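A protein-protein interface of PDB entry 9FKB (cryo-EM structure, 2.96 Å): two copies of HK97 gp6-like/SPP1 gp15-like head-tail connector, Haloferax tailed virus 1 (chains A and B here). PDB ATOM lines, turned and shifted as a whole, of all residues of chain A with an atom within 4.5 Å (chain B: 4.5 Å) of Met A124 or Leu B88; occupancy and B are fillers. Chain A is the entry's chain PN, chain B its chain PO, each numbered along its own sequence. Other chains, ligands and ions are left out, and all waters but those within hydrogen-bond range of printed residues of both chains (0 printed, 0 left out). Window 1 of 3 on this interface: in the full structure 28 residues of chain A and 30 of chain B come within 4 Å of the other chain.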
ATOM      1  N   TYR A  80      24.212  17.549  18.902  1.00  0.00           N
ATOM      2  CA  TYR A  80      25.424  17.010  19.513  1.00  0.00           C
ATOM      3  C   TYR A  80      26.681  17.484  18.784  1.00  0.00           C
ATOM      4  O   TYR A  80      27.642  17.896  19.418  1.00  0.00           O
ATOM      5  CB  TYR A  80      25.397  15.480  19.583  1.00  0.00           C
ATOM      6  CG  TYR A  80      24.431  14.898  20.583  1.00  0.00           C
ATOM      7  CD1 TYR A  80      24.464  15.299  21.909  1.00  0.00           C
ATOM      8  CD2 TYR A  80      23.464  13.971  20.218  1.00  0.00           C
ATOM      9  CE1 TYR A  80      23.553  14.833  22.848  1.00  0.00           C
ATOM     10  CE2 TYR A  80      22.543  13.506  21.150  1.00  0.00           C
ATOM     11  CZ  TYR A  80      22.586  13.918  22.466  1.00  0.00           C
ATOM     12  OH  TYR A  80      21.666  13.418  23.342  1.00  0.00           O
ATOM     13  N   ARG A 120      32.342  14.567  25.331  1.00  0.00           N
ATOM     14  CA  ARG A 120      31.087  13.922  25.718  1.00  0.00           C
ATOM     15  C   ARG A 120      30.015  14.057  24.631  1.00  0.00           C
ATOM     16  O   ARG A 120      29.362  13.073  24.272  1.00  0.00           O
ATOM     17  CB  ARG A 120      30.661  14.410  27.107  1.00  0.00           C
ATOM     18  CG  ARG A 120      30.242  15.875  27.198  1.00  0.00           C
ATOM     19  CD  ARG A 120      30.534  16.481  28.569  1.00  0.00           C
ATOM     20  NE  ARG A 120      29.976  17.824  28.688  1.00  0.00           N
ATOM     21  CZ  ARG A 120      30.611  18.975  28.926  1.00  0.00           C
ATOM     22  NH1 ARG A 120      29.904  20.084  29.019  1.00  0.00           N
ATOM     23  NH2 ARG A 120      31.914  19.041  29.131  1.00  0.00           N
ATOM     24  N   TYR A 121      29.895  15.257  24.050  1.00  0.00           N
ATOM     25  CA  TYR A 121      28.992  15.528  22.942  1.00  0.00           C
ATOM     26  C   TYR A 121      29.390  14.772  21.676  1.00  0.00           C
ATOM     27  O   TYR A 121      28.531  14.244  20.972  1.00  0.00           O
ATOM     28  CB  TYR A 121      28.889  17.032  22.715  1.00  0.00           C
ATOM     29  CG  TYR A 121      28.488  17.765  23.961  1.00  0.00           C
ATOM     30  CD1 TYR A 121      27.233  17.554  24.514  1.00  0.00           C
ATOM     31  CD2 TYR A 121      29.366  18.613  24.625  1.00  0.00           C
ATOM     32  CE1 TYR A 121      26.846  18.164  25.700  1.00  0.00           C
ATOM     33  CE2 TYR A 121      28.997  19.235  25.815  1.00  0.00           C
ATOM     34  CZ  TYR A 121      27.734  19.011  26.353  1.00  0.00           C
ATOM     35  OH  TYR A 121      27.338  19.626  27.510  1.00  0.00           O
ATOM     36  N   GLY A 122      30.695  14.684  21.405  1.00  0.00           N
ATOM     37  CA  GLY A 122      31.199  13.876  20.306  1.00  0.00           C
ATOM     38  C   GLY A 122      30.866  12.390  20.485  1.00  0.00           C
ATOM     39  O   GLY A 122      30.307  11.770  19.587  1.00  0.00           O
ATOM     40  N   ARG A 123      31.131  11.833  21.676  1.00  0.00           N
ATOM     41  CA  ARG A 123      30.869  10.435  21.993  1.00  0.00           C
ATOM     42  C   ARG A 123      29.380  10.096  21.920  1.00  0.00           C
ATOM     43  O   ARG A 123      29.031   9.003  21.498  1.00  0.00           O
ATOM     44  CB  ARG A 123      31.494  10.073  23.341  1.00  0.00           C
ATOM     45  CG  ARG A 123      33.014  10.015  23.288  1.00  0.00           C
ATOM     46  CD  ARG A 123      33.639   9.482  24.558  1.00  0.00           C
ATOM     47  NE  ARG A 123      33.524  10.326  25.743  1.00  0.00           N
ATOM     48  CZ  ARG A 123      34.476  11.091  26.272  1.00  0.00           C
ATOM     49  NH1 ARG A 123      34.230  11.742  27.397  1.00  0.00           N
ATOM     50  NH2 ARG A 123      35.668  11.199  25.705  1.00  0.00           N
ATOM     51  N   MET A 124      28.501  11.039  22.275  1.00  0.00           N
ATOM     52  CA  MET A 124      27.070  10.903  22.038  1.00  0.00           C
ATOM     53  C   MET A 124      26.736  10.893  20.541  1.00  0.00           C
ATOM     54  O   MET A 124      26.014  10.012  20.091  1.00  0.00           O
ATOM     55  CB  MET A 124      26.282  11.969  22.804  1.00  0.00           C
ATOM     56  CG  MET A 124      26.251  11.638  24.289  1.00  0.00           C
ATOM     57  SD  MET A 124      25.148  12.628  25.324  1.00  0.00           S
ATOM     58  CE  MET A 124      26.033  14.185  25.398  1.00  0.00           C
ATOM     59  N   ALA A 125      27.291  11.821  19.745  1.00  0.00           N
ATOM     60  CA  ALA A 125      27.073  11.859  18.297  1.00  0.00           C
ATOM     61  C   ALA A 125      27.599  10.611  17.571  1.00  0.00           C
ATOM     62  O   ALA A 125      27.030  10.179  16.577  1.00  0.00           O
ATOM     63  CB  ALA A 125      27.732  13.093  17.732  1.00  0.00           C
ATOM     64  N   LEU A 126      28.693  10.013  18.056  1.00  0.00           N
ATOM     65  CA  LEU A 126      29.425   8.958  17.364  1.00  0.00           C
ATOM     66  C   LEU A 126      28.577   7.699  17.116  1.00  0.00           C
ATOM     67  O   LEU A 126      28.701   7.074  16.064  1.00  0.00           O
ATOM     68  CB  LEU A 126      30.699   8.696  18.176  1.00  0.00           C
ATOM     69  CG  LEU A 126      31.726   7.739  17.578  1.00  0.00           C
ATOM     70  CD1 LEU A 126      32.146   8.157  16.166  1.00  0.00           C
ATOM     71  CD2 LEU A 126      32.961   7.678  18.480  1.00  0.00           C
ATOM     72  N   GLU A 127      27.665   7.358  18.034  1.00  0.00           N
ATOM     73  CA  GLU A 127      26.696   6.273  17.874  1.00  0.00           C
ATOM     74  C   GLU A 127      25.703   6.499  16.722  1.00  0.00           C
ATOM     75  O   GLU A 127      25.157   5.543  16.174  1.00  0.00           O
ATOM     76  CB  GLU A 127      25.947   5.995  19.181  1.00  0.00           C
ATOM     77  CG  GLU A 127      26.800   5.395  20.299  1.00  0.00           C
ATOM     78  CD  GLU A 127      27.148   3.908  20.233  1.00  0.00           C
ATOM     79  OE1 GLU A 127      26.746   3.215  19.271  1.00  0.00           O
ATOM     80  OE2 GLU A 127      27.854   3.419  21.139  1.00  0.00           O
ATOM     81  N   TYR A 128      25.452   7.762  16.346  1.00  0.00           N
ATOM     82  CA  TYR A 128      24.556   8.103  15.247  1.00  0.00           C
ATOM     83  C   TYR A 128      25.166   7.744  13.888  1.00  0.00           C
ATOM     84  O   TYR A 128      24.440   7.682  12.904  1.00  0.00           O
ATOM     85  CB  TYR A 128      24.188   9.597  15.294  1.00  0.00           C
ATOM     86  CG  TYR A 128      23.227   9.983  16.398  1.00  0.00           C
ATOM     87  CD1 TYR A 128      23.607   9.890  17.734  1.00  0.00           C
ATOM     88  CD2 TYR A 128      21.961  10.489  16.115  1.00  0.00           C
ATOM     89  CE1 TYR A 128      22.716  10.200  18.755  1.00  0.00           C
ATOM     90  CE2 TYR A 128      21.071  10.818  17.129  1.00  0.00           C
ATOM     91  CZ  TYR A 128      21.440  10.653  18.454  1.00  0.00           C
ATOM     92  OH  TYR A 128      20.554  10.961  19.450  1.00  0.00           O
ATOM     93  N   HIS B  84      21.459   9.443  31.948  1.00  0.00           N
ATOM     94  CA  HIS B  84      22.699   9.460  31.182  1.00  0.00           C
ATOM     95  C   HIS B  84      22.887  10.762  30.392  1.00  0.00           C
ATOM     96  O   HIS B  84      24.001  11.270  30.341  1.00  0.00           O
ATOM     97  CB  HIS B  84      22.717   8.235  30.269  1.00  0.00           C
ATOM     98  CG  HIS B  84      23.747   8.275  29.193  1.00  0.00           C
ATOM     99  ND1 HIS B  84      25.101   8.092  29.402  1.00  0.00           N
ATOM    100  CD2 HIS B  84      23.599   8.523  27.876  1.00  0.00           C
ATOM    101  CE1 HIS B  84      25.732   8.236  28.249  1.00  0.00           C
ATOM    102  NE2 HIS B  84      24.829   8.473  27.296  1.00  0.00           N
ATOM    103  N   LYS B  85      21.814  11.318  29.813  1.00  0.00           N
ATOM    104  CA  LYS B  85      21.824  12.574  29.066  1.00  0.00           C
ATOM    105  C   LYS B  85      21.619  13.836  29.921  1.00  0.00           C
ATOM    106  O   LYS B  85      21.809  14.939  29.417  1.00  0.00           O
ATOM    107  CB  LYS B  85      20.788  12.505  27.944  1.00  0.00           C
ATOM    108  CG  LYS B  85      21.316  11.839  26.684  1.00  0.00           C
ATOM    109  CD  LYS B  85      20.235  11.140  25.876  1.00  0.00           C
ATOM    110  CE  LYS B  85      20.544  10.898  24.408  1.00  0.00           C
ATOM    111  NZ  LYS B  85      21.915  10.401  24.128  1.00  0.00           N
ATOM    112  N   ILE B  86      21.213  13.712  31.197  1.00  0.00           N
ATOM    113  CA  ILE B  86      21.192  14.833  32.135  1.00  0.00           C
ATOM    114  C   ILE B  86      22.579  14.987  32.758  1.00  0.00           C
ATOM    115  O   ILE B  86      23.127  16.084  32.802  1.00  0.00           O
ATOM    116  CB  ILE B  86      20.056  14.672  33.164  1.00  0.00           C
ATOM    117  CG1 ILE B  86      18.705  14.838  32.463  1.00  0.00           C
ATOM    118  CG2 ILE B  86      20.203  15.656  34.319  1.00  0.00           C
ATOM    119  CD1 ILE B  86      17.503  14.373  33.252  1.00  0.00           C
ATOM    120  N   GLN B  87      23.199  13.873  33.158  1.00  0.00           N
ATOM    121  CA  GLN B  87      24.652  13.801  33.174  1.00  0.00           C
ATOM    122  C   GLN B  87      25.176  14.111  31.761  1.00  0.00           C
ATOM    123  O   GLN B  87      24.418  14.142  30.801  1.00  0.00           O
ATOM    124  CB  GLN B  87      25.093  12.422  33.667  1.00  0.00           C
ATOM    125  CG  GLN B  87      26.386  12.444  34.486  1.00  0.00           C
ATOM    126  CD  GLN B  87      26.219  13.061  35.857  1.00  0.00           C
ATOM    127  OE1 GLN B  87      25.153  12.971  36.451  1.00  0.00           O
ATOM    128  NE2 GLN B  87      27.267  13.680  36.386  1.00  0.00           N
ATOM    129  N   LEU B  88      26.471  14.391  31.613  1.00  0.00           N
ATOM    130  CA  LEU B  88      27.056  14.858  30.352  1.00  0.00           C
ATOM    131  C   LEU B  88      26.595  16.271  29.942  1.00  0.00           C
ATOM    132  O   LEU B  88      27.428  17.048  29.480  1.00  0.00           O
ATOM    133  CB  LEU B  88      26.953  13.817  29.223  1.00  0.00           C
ATOM    134  CG  LEU B  88      27.314  12.370  29.577  1.00  0.00           C
ATOM    135  CD1 LEU B  88      27.270  11.494  28.336  1.00  0.00           C
ATOM    136  CD2 LEU B  88      28.696  12.272  30.211  1.00  0.00           C
ATOM    137  N   PHE B  89      25.327  16.660  30.157  1.00  0.00           N
ATOM    138  CA  PHE B  89      24.958  18.076  30.188  1.00  0.00           C
ATOM    139  C   PHE B  89      25.527  18.767  31.443  1.00  0.00           C
ATOM    140  O   PHE B  89      25.507  19.990  31.552  1.00  0.00           O
ATOM    141  CB  PHE B  89      23.437  18.278  30.078  1.00  0.00           C
ATOM    142  CG  PHE B  89      22.708  17.863  28.812  1.00  0.00           C
ATOM    143  CD1 PHE B  89      23.298  17.086  27.814  1.00  0.00           C
ATOM    144  CD2 PHE B  89      21.377  18.224  28.635  1.00  0.00           C
ATOM    145  CE1 PHE B  89      22.593  16.725  26.665  1.00  0.00           C
ATOM    146  CE2 PHE B  89      20.660  17.841  27.503  1.00  0.00           C
ATOM    147  CZ  PHE B  89      21.266  17.085  26.521  1.00  0.00           C
ATOM    148  N   GLU B  90      26.064  17.996  32.401  1.00  0.00           N
ATOM    149  CA  GLU B  90      26.755  18.496  33.590  1.00  0.00           C
ATOM    150  C   GLU B  90      28.212  18.024  33.677  1.00  0.00           C
ATOM    151  O   GLU B  90      28.771  17.936  34.775  1.00  0.00           O
ATOM    152  CB  GLU B  90      25.992  18.034  34.831  1.00  0.00           C
ATOM    153  CG  GLU B  90      24.597  18.626  34.935  1.00  0.00           C
ATOM    154  CD  GLU B  90      23.932  18.396  36.286  1.00  0.00           C
ATOM    155  OE1 GLU B  90      24.454  17.573  37.072  1.00  0.00           O
ATOM    156  OE2 GLU B  90      22.896  19.046  36.558  1.00  0.00           O
ATOM    157  N   GLY B  91      28.842  17.728  32.531  1.00  0.00           N
ATOM    158  CA  GLY B  91      30.130  17.047  32.512  1.00  0.00           C
ATOM    159  C   GLY B  91      30.022  15.568  32.909  1.00  0.00           C
ATOM    160  O   GLY B  91      28.930  15.003  32.990  1.00  0.00           O
ATOM    161  N   GLY B  92      31.177  14.925  33.134  1.00  0.00           N
ATOM    162  CA  GLY B  92      31.242  13.482  33.358  1.00  0.00           C
ATOM    163  C   GLY B  92      30.800  13.038  34.755  1.00  0.00           C
ATOM    164  O   GLY B  92      30.058  13.731  35.453  1.00  0.00           O
ATOM    165  N   ASP B 115      29.931   6.288  24.937  1.00  0.00           N
ATOM    166  CA  ASP B 115      29.210   7.143  25.878  1.00  0.00           C
ATOM    167  C   ASP B 115      28.492   6.327  26.966  1.00  0.00           C
ATOM    168  O   ASP B 115      28.578   6.680  28.149  1.00  0.00           O
ATOM    169  CB  ASP B 115      28.295   8.155  25.182  1.00  0.00           C
ATOM    170  CG  ASP B 115      27.028   7.541  24.620  1.00  0.00           C
ATOM    171  OD1 ASP B 115      27.108   6.401  24.122  1.00  0.00           O
ATOM    172  OD2 ASP B 115      25.968   8.189  24.721  1.00  0.00           O
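Of chain B, only Leu B88 and Asp B115 come within 4 Å of Met A124.
Leu B88 touches three residues of chain A.
Printed residues of chain A within 4 Å of Phe B89: Tyr A121.
Of the printed residues of chain B, Arg A120 touches Leu B88 and Gly B91.
Leu A126 touches none of the printed residues of chain B.
Ile B86 touches none of the printed residues of chain A.
The nearest residue of chain B that does not touch Met A124 is Lys B85 (4.1 Å).
The nearest printed residue of chain A that does not touch Leu B88 is Arg A123 (6.2 Å).
Along chain B the printed residues that touch a printed residue of chain A span positions 85 to 115.
Of the 10 printed residues of chain A, 6 touch a printed residue of chain B.
Hydrophobic or aromatic side chains of chain A that line the printed part of chain B: Tyr A80, Tyr A121 and Met A124.
Among the printed residues, 9 pairs touch across the chains.
The side-chain hydroxyl (OH) of Tyr A80 lies close to the side-chain amino group (NZ) of Lys B85, 3.1 Å away.
The guanidinium group (NE) of Arg A120 lies within hydrogen-bond range of the backbone carbonyl oxygen (O) of Leu B88 (2.8 Å).
O of Leu B88 sits at hydrogen-bond distance from OH of Tyr A121 (3.2 Å).
No position is printed for both chains.
Of the 9 pairs that touch across the chains among the printed residues, none has its exchanged pair printed and touching as well.
OH of Tyr A121 is in hydrogen-bond range of NH1 of Arg A120, 3.0 Å away.
A ring nitrogen (NE2) of His B84 sits at hydrogen-bond distance from the side-chain carboxylate of Asp B115 (2.8 Å).
Arg A120 touches Gly B91.
Tyr A121 touches Phe B89.
Arg A123 touches Asp B115 (O to CB, 3.9 Å).
Met A124 touches Leu B88 (SD to CD1, 3.9 Å).
Met A124 touches Asp B115.
CG of Glu A127 touches OD1 of Asp B115, 3.97 Å away.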
